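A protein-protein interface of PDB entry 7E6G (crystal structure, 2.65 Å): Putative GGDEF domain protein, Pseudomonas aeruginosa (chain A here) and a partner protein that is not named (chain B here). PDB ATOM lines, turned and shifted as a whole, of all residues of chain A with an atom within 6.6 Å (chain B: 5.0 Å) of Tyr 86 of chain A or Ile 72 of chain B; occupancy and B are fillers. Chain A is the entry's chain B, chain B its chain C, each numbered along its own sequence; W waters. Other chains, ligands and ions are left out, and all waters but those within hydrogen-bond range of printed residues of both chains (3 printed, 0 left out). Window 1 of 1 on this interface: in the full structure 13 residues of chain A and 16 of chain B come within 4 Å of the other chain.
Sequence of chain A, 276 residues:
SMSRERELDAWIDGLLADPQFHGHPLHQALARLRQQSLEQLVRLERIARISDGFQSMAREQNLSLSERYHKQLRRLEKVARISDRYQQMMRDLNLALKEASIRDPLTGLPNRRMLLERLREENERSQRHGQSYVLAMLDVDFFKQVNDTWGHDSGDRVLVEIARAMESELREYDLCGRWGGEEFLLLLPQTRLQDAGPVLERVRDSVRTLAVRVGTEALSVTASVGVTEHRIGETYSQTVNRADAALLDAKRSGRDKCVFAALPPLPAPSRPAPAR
OG1 of Thr 69 of chain B is in hydrogen-bond range of OG of Ser 83 of chain A (2.6 Å).
The side-chain sulfur (SD) of Met 90 of chain A sits at hydrogen-bond distance from the side-chain hydroxyl (OH) of Tyr 66 of chain B (3.7 Å).
OG of Ser 83 of chain A is in hydrogen-bond range of NE2 of Gln 87 of chain A (3.3 Å).
Among the printed residues, merely in contact across the chains: Val 79 of chain A with Thr 69 of chain B (3.6 Å), Ile 82 of chain A with Ile 72 of chain B (3.8 Å), Ser 83 of chain A with Ile 72 of chain B (3.5 Å), Arg 85 of chain A with Leu 108 of chain B (3.6 Å), Tyr 86 of chain A with Leu 65 of chain B (3.8 Å), Tyr 86 of chain A with Tyr 66 of chain B (3.4 Å), Tyr 86 of chain A with Leu 67 of chain B (3.3 Å), Tyr 86 of chain A with Ile 72 of chain B (3.7 Å), Tyr 86 of chain A with Trp 96 of chain B (3.9 Å), Tyr 86 of chain A with Leu 108 of chain B (3.3 Å), Tyr 86 of chain A with Phe 112 of chain B (3.9 Å) and Gln 87 of chain A with Tyr 66 of chain B (3.6 Å).
Asp 84 of chain A touches none of the printed residues of chain B.
Of the printed residues of chain B, Tyr 86 of chain A touches Leu 65 (3.8 Å), Tyr 66 (3.4 Å), Leu 67 (3.3 Å), Ile 72 (3.7 Å), Trp 96 (3.9 Å), Leu 108 (3.3 Å) and Phe 112 (3.9 Å).
Printed residues of chain B within 4 Å of Met 90 of chain A: Tyr 66.
Printed residues of chain A within 4 Å of Leu 65 of chain B: Tyr 86.
Printed residues of chain A within 4 Å of Tyr 66 of chain B: Tyr 86 (3.4 Å), Gln 87 (3.6 Å) and Met 90 (3.7 Å).
Ile 72 of chain B touches just these residues of chain A: Ile 82 (3.8 Å), Ser 83 (3.5 Å) and Tyr 86 (3.7 Å).
The nearest residue of chain A that does not touch Ile 72 of chain B is Val 79 of chain A (4.3 Å).
The nearest printed residue of chain B that does not touch Gln 87 of chain A is Thr 69 of chain B (4.3 Å).
Of the 15 printed residues of chain B, 8 touch a printed residue of chain A.
Of the 14 printed residues of chain A, 7 touch a printed residue of chain B.
Printed residues of chain A that touch a printed residue of chain B: Val 79, Ile 82, Ser 83, Arg 85, Tyr 86, Gln 87 and Met 90.
Hydrophobic or aromatic side chains of chain A that line the printed part of chain B: Val 79, Ile 82, Tyr 86 and Met 90.
Among the printed residues, 14 pairs touch across the chains.
Among the printed residues, no Asp or Glu carboxylate lies within 4 Å of a Lys or Arg side-chain nitrogen of the other chain.
Water W1 bridges OG of Ser 83 of chain A (2.5 Å) and O of Leu 67 of chain B (2.9 Å).
Water W2 lies within hydrogen-bond range of O of Leu 65 of chain B (2.7 Å) and OH of Tyr 86 of chain A (2.9 Å).
Water W3 lies within hydrogen-bond range of NZ of Lys 78 of chain A and O of Phe 112 of chain B.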
ATOM      1  N   LYS A  78     -23.374  15.498   0.344  1.00  0.00           N
ATOM      2  CA  LYS A  78     -23.134  16.866  -0.112  1.00  0.00           C
ATOM      3  C   LYS A  78     -22.437  16.908  -1.477  1.00  0.00           C
ATOM      4  O   LYS A  78     -22.810  17.703  -2.360  1.00  0.00           O
ATOM      5  CB  LYS A  78     -22.310  17.620   0.934  1.00  0.00           C
ATOM      6  CG  LYS A  78     -22.110  19.080   0.618  1.00  0.00           C
ATOM      7  CD  LYS A  78     -21.362  19.787   1.718  1.00  0.00           C
ATOM      8  CE  LYS A  78     -21.503  21.294   1.586  1.00  0.00           C
ATOM      9  NZ  LYS A  78     -21.069  22.067   2.805  1.00  0.00           N
ATOM     10  N   VAL A  79     -21.387  16.103  -1.655  1.00  0.00           N
ATOM     11  CA  VAL A  79     -20.740  16.030  -2.963  1.00  0.00           C
ATOM     12  C   VAL A  79     -21.770  15.720  -4.050  1.00  0.00           C
ATOM     13  O   VAL A  79     -21.817  16.393  -5.092  1.00  0.00           O
ATOM     14  CB  VAL A  79     -19.607  14.989  -2.956  1.00  0.00           C
ATOM     15  CG1 VAL A  79     -19.196  14.648  -4.376  1.00  0.00           C
ATOM     16  CG2 VAL A  79     -18.421  15.491  -2.173  1.00  0.00           C
ATOM     17  N   ALA A  80     -22.617  14.701  -3.818  1.00  0.00           N
ATOM     18  CA  ALA A  80     -23.616  14.340  -4.822  1.00  0.00           C
ATOM     19  C   ALA A  80     -24.598  15.482  -5.093  1.00  0.00           C
ATOM     20  O   ALA A  80     -24.944  15.747  -6.252  1.00  0.00           O
ATOM     21  CB  ALA A  80     -24.366  13.083  -4.385  1.00  0.00           C
ATOM     22  N   ARG A  81     -25.050  16.183  -4.046  1.00  0.00           N
ATOM     23  CA  ARG A  81     -25.975  17.302  -4.248  1.00  0.00           C
ATOM     24  C   ARG A  81     -25.375  18.393  -5.140  1.00  0.00           C
ATOM     25  O   ARG A  81     -25.988  18.819  -6.137  1.00  0.00           O
ATOM     26  CB  ARG A  81     -26.371  17.876  -2.894  1.00  0.00           C
ATOM     27  CG  ARG A  81     -27.490  18.878  -2.980  1.00  0.00           C
ATOM     28  CD  ARG A  81     -27.848  19.446  -1.617  1.00  0.00           C
ATOM     29  NE  ARG A  81     -27.351  18.607  -0.533  1.00  0.00           N
ATOM     30  CZ  ARG A  81     -26.578  19.057   0.450  1.00  0.00           C
ATOM     31  NH1 ARG A  81     -26.230  20.337   0.480  1.00  0.00           N
ATOM     32  NH2 ARG A  81     -26.156  18.229   1.400  1.00  0.00           N
ATOM     33  N   ILE A  82     -24.169  18.856  -4.797  1.00  0.00           N
ATOM     34  CA  ILE A  82     -23.534  19.920  -5.575  1.00  0.00           C
ATOM     35  C   ILE A  82     -23.296  19.470  -7.009  1.00  0.00           C
ATOM     36  O   ILE A  82     -23.557  20.212  -7.973  1.00  0.00           O
ATOM     37  CB  ILE A  82     -22.213  20.355  -4.920  1.00  0.00           C
ATOM     38  CG1 ILE A  82     -22.473  21.036  -3.578  1.00  0.00           C
ATOM     39  CG2 ILE A  82     -21.438  21.271  -5.853  1.00  0.00           C
ATOM     40  CD1 ILE A  82     -21.238  21.143  -2.684  1.00  0.00           C
ATOM     41  N   SER A  83     -22.738  18.264  -7.170  1.00  0.00           N
ATOM     42  CA  SER A  83     -22.492  17.739  -8.506  1.00  0.00           C
ATOM     43  C   SER A  83     -23.771  17.715  -9.331  1.00  0.00           C
ATOM     44  O   SER A  83     -23.765  18.141 -10.493  1.00  0.00           O
ATOM     45  CB  SER A  83     -21.885  16.346  -8.410  1.00  0.00           C
ATOM     46  OG  SER A  83     -21.116  16.050  -9.553  1.00  0.00           O
ATOM     47  N   ASP A  84     -24.881  17.239  -8.743  1.00  0.00           N
ATOM     48  CA  ASP A  84     -26.154  17.211  -9.458  1.00  0.00           C
ATOM     49  C   ASP A  84     -26.525  18.596  -9.972  1.00  0.00           C
ATOM     50  O   ASP A  84     -27.059  18.739 -11.077  1.00  0.00           O
ATOM     51  CB  ASP A  84     -27.260  16.689  -8.550  1.00  0.00           C
ATOM     52  CG  ASP A  84     -27.128  15.205  -8.211  1.00  0.00           C
ATOM     53  OD1 ASP A  84     -26.469  14.408  -8.926  1.00  0.00           O
ATOM     54  OD2 ASP A  84     -27.705  14.818  -7.177  1.00  0.00           O
ATOM     55  N   ARG A  85     -26.254  19.633  -9.186  1.00  0.00           N
ATOM     56  CA  ARG A  85     -26.598  20.967  -9.668  1.00  0.00           C
ATOM     57  C   ARG A  85     -25.714  21.388 -10.846  1.00  0.00           C
ATOM     58  O   ARG A  85     -26.217  21.927 -11.859  1.00  0.00           O
ATOM     59  CB  ARG A  85     -26.544  21.940  -8.505  1.00  0.00           C
ATOM     60  CG  ARG A  85     -27.673  21.636  -7.528  1.00  0.00           C
ATOM     61  CD  ARG A  85     -27.549  22.406  -6.245  1.00  0.00           C
ATOM     62  NE  ARG A  85     -27.896  23.805  -6.446  1.00  0.00           N
ATOM     63  CZ  ARG A  85     -28.145  24.650  -5.456  1.00  0.00           C
ATOM     64  NH1 ARG A  85     -28.068  24.220  -4.194  1.00  0.00           N
ATOM     65  NH2 ARG A  85     -28.457  25.917  -5.733  1.00  0.00           N
ATOM     66  N   TYR A  86     -24.401  21.118 -10.764  1.00  0.00           N
ATOM     67  CA  TYR A  86     -23.544  21.368 -11.934  1.00  0.00           C
ATOM     68  C   TYR A  86     -24.073  20.637 -13.168  1.00  0.00           C
ATOM     69  O   TYR A  86     -24.091  21.185 -14.285  1.00  0.00           O
ATOM     70  CB  TYR A  86     -22.103  20.934 -11.658  1.00  0.00           C
ATOM     71  CG  TYR A  86     -21.290  21.970 -10.933  1.00  0.00           C
ATOM     72  CD1 TYR A  86     -20.644  22.980 -11.629  1.00  0.00           C
ATOM     73  CD2 TYR A  86     -21.186  21.955  -9.547  1.00  0.00           C
ATOM     74  CE1 TYR A  86     -19.907  23.937 -10.976  1.00  0.00           C
ATOM     75  CE2 TYR A  86     -20.439  22.908  -8.884  1.00  0.00           C
ATOM     76  CZ  TYR A  86     -19.806  23.897  -9.615  1.00  0.00           C
ATOM     77  OH  TYR A  86     -19.069  24.857  -8.977  1.00  0.00           O
ATOM     78  N   GLN A  87     -24.526  19.399 -12.978  1.00  0.00           N
ATOM     79  CA  GLN A  87     -24.968  18.618 -14.119  1.00  0.00           C
ATOM     80  C   GLN A  87     -26.296  19.131 -14.653  1.00  0.00           C
ATOM     81  O   GLN A  87     -26.599  18.957 -15.841  1.00  0.00           O
ATOM     82  CB  GLN A  87     -25.054  17.148 -13.738  1.00  0.00           C
ATOM     83  CG  GLN A  87     -23.694  16.524 -13.607  1.00  0.00           C
ATOM     84  CD  GLN A  87     -23.768  15.149 -12.998  1.00  0.00           C
ATOM     85  OE1 GLN A  87     -24.146  14.178 -13.671  1.00  0.00           O
ATOM     86  NE2 GLN A  87     -23.426  15.050 -11.710  1.00  0.00           N
ATOM     87  N   GLN A  88     -27.088  19.769 -13.796  1.00  0.00           N
ATOM     88  CA  GLN A  88     -28.284  20.438 -14.276  1.00  0.00           C
ATOM     89  C   GLN A  88     -27.918  21.540 -15.264  1.00  0.00           C
ATOM     90  O   GLN A  88     -28.590  21.724 -16.291  1.00  0.00           O
ATOM     91  CB  GLN A  88     -29.078  20.988 -13.093  1.00  0.00           C
ATOM     92  CG  GLN A  88     -30.470  21.480 -13.448  1.00  0.00           C
ATOM     93  CD  GLN A  88     -31.238  20.510 -14.340  1.00  0.00           C
ATOM     94  OE1 GLN A  88     -31.550  20.820 -15.500  1.00  0.00           O
ATOM     95  NE2 GLN A  88     -31.556  19.333 -13.798  1.00  0.00           N
ATOM     96  N   MET A  89     -26.842  22.275 -14.990  1.00  0.00           N
ATOM     97  CA  MET A  89     -26.444  23.284 -15.979  1.00  0.00           C
ATOM     98  C   MET A  89     -25.970  22.633 -17.279  1.00  0.00           C
ATOM     99  O   MET A  89     -26.247  23.120 -18.389  1.00  0.00           O
ATOM    100  CB  MET A  89     -25.347  24.181 -15.423  1.00  0.00           C
ATOM    101  CG  MET A  89     -25.594  24.665 -14.015  1.00  0.00           C
ATOM    102  SD  MET A  89     -24.369  25.915 -13.584  1.00  0.00           S
ATOM    103  CE  MET A  89     -22.861  25.232 -14.302  1.00  0.00           C
ATOM    104  N   MET A  90     -25.229  21.540 -17.158  1.00  0.00           N
ATOM    105  CA  MET A  90     -24.772  20.836 -18.357  1.00  0.00           C
ATOM    106  C   MET A  90     -25.950  20.302 -19.170  1.00  0.00           C
ATOM    107  O   MET A  90     -25.910  20.253 -20.407  1.00  0.00           O
ATOM    108  CB  MET A  90     -23.845  19.705 -17.932  1.00  0.00           C
ATOM    109  CG  MET A  90     -23.043  19.082 -19.021  1.00  0.00           C
ATOM    110  SD  MET A  90     -21.987  17.830 -18.259  1.00  0.00           S
ATOM    111  CE  MET A  90     -20.411  18.258 -18.975  1.00  0.00           C
ATOM    112  N   ARG A  91     -27.023  19.914 -18.482  1.00  0.00           N
ATOM    113  CA  ARG A  91     -28.226  19.439 -19.151  1.00  0.00           C
ATOM    114  C   ARG A  91     -28.967  20.575 -19.849  1.00  0.00           C
ATOM    115  O   ARG A  91     -29.527  20.386 -20.936  1.00  0.00           O
ATOM    116  CB  ARG A  91     -29.136  18.762 -18.133  1.00  0.00           C
ATOM    117  CG  ARG A  91     -30.149  17.842 -18.739  1.00  0.00           C
ATOM    118  CD  ARG A  91     -31.453  17.826 -17.954  1.00  0.00           C
ATOM    119  NE  ARG A  91     -32.242  16.719 -18.471  1.00  0.00           N
ATOM    120  CZ  ARG A  91     -33.547  16.739 -18.721  1.00  0.00           C
ATOM    121  NH1 ARG A  91     -34.281  17.834 -18.488  1.00  0.00           N
ATOM    122  NH2 ARG A  91     -34.105  15.638 -19.222  1.00  0.00           N
ATOM    123  N   LEU B  65     -14.787  27.364 -13.290  1.00  0.00           N
ATOM    124  CA  LEU B  65     -15.934  27.145 -14.054  1.00  0.00           C
ATOM    125  C   LEU B  65     -16.625  25.829 -13.824  1.00  0.00           C
ATOM    126  O   LEU B  65     -17.091  25.633 -12.824  1.00  0.00           O
ATOM    127  CB  LEU B  65     -15.609  27.345 -15.477  1.00  0.00           C
ATOM    128  CG  LEU B  65     -14.912  28.628 -15.727  1.00  0.00           C
ATOM    129  CD1 LEU B  65     -14.233  28.707 -16.994  1.00  0.00           C
ATOM    130  CD2 LEU B  65     -15.803  29.754 -15.596  1.00  0.00           C
ATOM    131  N   TYR B  66     -16.713  24.937 -14.739  1.00  0.00           N
ATOM    132  CA  TYR B  66     -17.372  23.687 -14.462  1.00  0.00           C
ATOM    133  C   TYR B  66     -16.535  22.760 -13.693  1.00  0.00           C
ATOM    134  O   TYR B  66     -15.447  22.661 -13.923  1.00  0.00           O
ATOM    135  CB  TYR B  66     -18.057  23.079 -15.649  1.00  0.00           C
ATOM    136  CG  TYR B  66     -18.818  21.834 -15.382  1.00  0.00           C
ATOM    137  CD1 TYR B  66     -18.197  20.621 -15.294  1.00  0.00           C
ATOM    138  CD2 TYR B  66     -20.148  21.860 -15.286  1.00  0.00           C
ATOM    139  CE1 TYR B  66     -18.908  19.502 -15.073  1.00  0.00           C
ATOM    140  CE2 TYR B  66     -20.841  20.729 -15.085  1.00  0.00           C
ATOM    141  CZ  TYR B  66     -20.223  19.574 -14.977  1.00  0.00           C
ATOM    142  OH  TYR B  66     -21.017  18.587 -14.773  1.00  0.00           O
ATOM    143  N   LEU B  67     -17.133  22.084 -12.766  1.00  0.00           N
ATOM    144  CA  LEU B  67     -16.449  21.198 -11.834  1.00  0.00           C
ATOM    145  C   LEU B  67     -17.133  19.840 -11.857  1.00  0.00           C
ATOM    146  O   LEU B  67     -18.294  19.734 -11.454  1.00  0.00           O
ATOM    147  CB  LEU B  67     -16.507  21.776 -10.413  1.00  0.00           C
ATOM    148  CG  LEU B  67     -15.532  22.861  -9.971  1.00  0.00           C
ATOM    149  CD1 LEU B  67     -15.317  23.859 -11.072  1.00  0.00           C
ATOM    150  CD2 LEU B  67     -16.089  23.532  -8.743  1.00  0.00           C
ATOM    151  N   ASN B  68     -16.422  18.800 -12.278  1.00  0.00           N
ATOM    152  CA  ASN B  68     -16.993  17.458 -12.206  1.00  0.00           C
ATOM    153  C   ASN B  68     -16.984  16.988 -10.747  1.00  0.00           C
ATOM    154  O   ASN B  68     -16.661  17.738  -9.821  1.00  0.00           O
ATOM    155  CB  ASN B  68     -16.282  16.501 -13.168  1.00  0.00           C
ATOM    156  CG  ASN B  68     -14.854  16.114 -12.726  1.00  0.00           C
ATOM    157  OD1 ASN B  68     -14.348  16.558 -11.691  1.00  0.00           O
ATOM    158  ND2 ASN B  68     -14.212  15.255 -13.529  1.00  0.00           N
ATOM    159  N   THR B  69     -17.335  15.726 -10.520  1.00  0.00           N
ATOM    160  CA  THR B  69     -17.627  15.280  -9.159  1.00  0.00           C
ATOM    161  C   THR B  69     -16.356  15.085  -8.335  1.00  0.00           C
ATOM    162  O   THR B  69     -16.283  15.516  -7.172  1.00  0.00           O
ATOM    163  CB  THR B  69     -18.447  13.992  -9.194  1.00  0.00           C
ATOM    164  OG1 THR B  69     -19.482  14.113 -10.191  1.00  0.00           O
ATOM    165  CG2 THR B  69     -19.071  13.748  -7.832  1.00  0.00           C
ATOM    166  N   SER B  70     -15.347  14.426  -8.906  1.00  0.00           N
ATOM    167  CA  SER B  70     -14.091  14.332  -8.171  1.00  0.00           C
ATOM    168  C   SER B  70     -13.513  15.708  -7.858  1.00  0.00           C
ATOM    169  O   SER B  70     -12.941  15.904  -6.785  1.00  0.00           O
ATOM    170  CB  SER B  70     -13.094  13.502  -8.956  1.00  0.00           C
ATOM    171  OG  SER B  70     -13.302  12.140  -8.646  1.00  0.00           O
ATOM    172  N   SER B  71     -13.696  16.676  -8.749  1.00  0.00           N
ATOM    173  CA  SER B  71     -13.200  18.024  -8.497  1.00  0.00           C
ATOM    174  C   SER B  71     -13.932  18.678  -7.323  1.00  0.00           C
ATOM    175  O   SER B  71     -13.303  19.299  -6.457  1.00  0.00           O
ATOM    176  CB  SER B  71     -13.348  18.870  -9.766  1.00  0.00           C
ATOM    177  OG  SER B  71     -12.545  18.353 -10.807  1.00  0.00           O
ATOM    178  N   ILE B  72     -15.267  18.592  -7.309  1.00  0.00           N
ATOM    179  CA  ILE B  72     -16.038  19.048  -6.155  1.00  0.00           C
ATOM    180  C   ILE B  72     -15.510  18.411  -4.875  1.00  0.00           C
ATOM    181  O   ILE B  72     -15.314  19.096  -3.861  1.00  0.00           O
ATOM    182  CB  ILE B  72     -17.538  18.746  -6.365  1.00  0.00           C
ATOM    183  CG1 ILE B  72     -18.122  19.651  -7.450  1.00  0.00           C
ATOM    184  CG2 ILE B  72     -18.330  18.911  -5.073  1.00  0.00           C
ATOM    185  CD1 ILE B  72     -19.293  19.061  -8.145  1.00  0.00           C
ATOM    186  N   LYS B  73     -15.274  17.090  -4.900  1.00  0.00           N
ATOM    187  CA  LYS B  73     -14.733  16.400  -3.731  1.00  0.00           C
ATOM    188  C   LYS B  73     -13.407  17.011  -3.293  1.00  0.00           C
ATOM    189  O   LYS B  73     -13.209  17.304  -2.106  1.00  0.00           O
ATOM    190  CB  LYS B  73     -14.551  14.914  -4.029  1.00  0.00           C
ATOM    191  CG  LYS B  73     -14.467  14.039  -2.793  1.00  0.00           C
ATOM    192  CD  LYS B  73     -13.055  13.521  -2.543  1.00  0.00           C
ATOM    193  CE  LYS B  73     -12.938  12.907  -1.139  1.00  0.00           C
ATOM    194  NZ  LYS B  73     -11.567  12.393  -0.878  1.00  0.00           N
ATOM    195  N   ALA B  74     -12.484  17.214  -4.241  1.00  0.00           N
ATOM    196  CA  ALA B  74     -11.166  17.738  -3.882  1.00  0.00           C
ATOM    197  C   ALA B  74     -11.260  19.156  -3.336  1.00  0.00           C
ATOM    198  O   ALA B  74     -10.526  19.531  -2.415  1.00  0.00           O
ATOM    199  CB  ALA B  74     -10.223  17.698  -5.087  1.00  0.00           C
ATOM    200  N   MET B  75     -12.141  19.966  -3.914  1.00  0.00           N
ATOM    201  CA  MET B  75     -12.361  21.308  -3.406  1.00  0.00           C
ATOM    202  C   MET B  75     -12.865  21.265  -1.971  1.00  0.00           C
ATOM    203  O   MET B  75     -12.432  22.053  -1.124  1.00  0.00           O
ATOM    204  CB  MET B  75     -13.345  22.034  -4.318  1.00  0.00           C
ATOM    205  CG  MET B  75     -13.085  23.512  -4.431  1.00  0.00           C
ATOM    206  SD  MET B  75     -11.420  23.901  -5.049  1.00  0.00           S
ATOM    207  CE  MET B  75     -11.179  22.641  -6.315  1.00  0.00           C
ATOM    208  N   MET B  76     -13.751  20.326  -1.667  1.00  0.00           N
ATOM    209  CA  MET B  76     -14.184  20.178  -0.286  1.00  0.00           C
ATOM    210  C   MET B  76     -13.039  19.743   0.617  1.00  0.00           C
ATOM    211  O   MET B  76     -12.969  20.147   1.783  1.00  0.00           O
ATOM    212  CB  MET B  76     -15.325  19.191  -0.232  1.00  0.00           C
ATOM    213  CG  MET B  76     -16.378  19.608  -1.177  1.00  0.00           C
ATOM    214  SD  MET B  76     -17.882  19.663  -0.271  1.00  0.00           S
ATOM    215  CE  MET B  76     -17.500  20.954   0.915  1.00  0.00           C
ATOM    216  N   TRP B  96     -14.473  33.566  -4.092  1.00  0.00           N
ATOM    217  CA  TRP B  96     -15.015  32.826  -5.225  1.00  0.00           C
ATOM    218  C   TRP B  96     -15.549  33.829  -6.244  1.00  0.00           C
ATOM    219  O   TRP B  96     -16.562  34.496  -5.988  1.00  0.00           O
ATOM    220  CB  TRP B  96     -16.124  31.878  -4.752  1.00  0.00           C
ATOM    221  CG  TRP B  96     -16.546  30.826  -5.778  1.00  0.00           C
ATOM    222  CD1 TRP B  96     -17.210  31.040  -6.959  1.00  0.00           C
ATOM    223  CD2 TRP B  96     -16.333  29.411  -5.694  1.00  0.00           C
ATOM    224  NE1 TRP B  96     -17.407  29.850  -7.614  1.00  0.00           N
ATOM    225  CE2 TRP B  96     -16.884  28.833  -6.859  1.00  0.00           C
ATOM    226  CE3 TRP B  96     -15.735  28.577  -4.744  1.00  0.00           C
ATOM    227  CZ2 TRP B  96     -16.847  27.463  -7.104  1.00  0.00           C
ATOM    228  CZ3 TRP B  96     -15.703  27.216  -4.991  1.00  0.00           C
ATOM    229  CH2 TRP B  96     -16.255  26.674  -6.160  1.00  0.00           C
ATOM    230  N   LEU B 108     -24.319  27.496  -6.108  1.00  0.00           N
ATOM    231  CA  LEU B 108     -23.322  26.434  -5.982  1.00  0.00           C
ATOM    232  C   LEU B 108     -22.241  26.830  -4.982  1.00  0.00           C
ATOM    233  O   LEU B 108     -21.909  26.075  -4.055  1.00  0.00           O
ATOM    234  CB  LEU B 108     -22.702  26.139  -7.357  1.00  0.00           C
ATOM    235  CG  LEU B 108     -23.294  25.063  -8.283  1.00  0.00           C
ATOM    236  CD1 LEU B 108     -24.810  25.053  -8.216  1.00  0.00           C
ATOM    237  CD2 LEU B 108     -22.836  25.244  -9.743  1.00  0.00           C
ATOM    238  N   PHE B 112     -20.898  25.495  -1.324  1.00  0.00           N
ATOM    239  CA  PHE B 112     -19.506  25.258  -0.928  1.00  0.00           C
ATOM    240  C   PHE B 112     -19.169  25.927   0.411  1.00  0.00           C
ATOM    241  O   PHE B 112     -18.354  25.402   1.187  1.00  0.00           O
ATOM    242  CB  PHE B 112     -18.549  25.755  -2.018  1.00  0.00           C
ATOM    243  CG  PHE B 112     -18.196  24.712  -3.038  1.00  0.00           C
ATOM    244  CD1 PHE B 112     -17.409  23.620  -2.690  1.00  0.00           C
ATOM    245  CD2 PHE B 112     -18.659  24.819  -4.342  1.00  0.00           C
ATOM    246  CE1 PHE B 112     -17.088  22.654  -3.617  1.00  0.00           C
ATOM    247  CE2 PHE B 112     -18.345  23.855  -5.283  1.00  0.00           C
ATOM    248  CZ  PHE B 112     -17.557  22.763  -4.920  1.00  0.00           C
HETATM  249  O   HOH W   1     -20.382  17.662 -11.371  1.00  0.00           O
HETATM  250  O   HOH W   2     -17.651  26.838 -10.516  1.00  0.00           O
HETATM  251  O   HOH W   3     -18.906  23.634   3.429  1.00  0.00           O
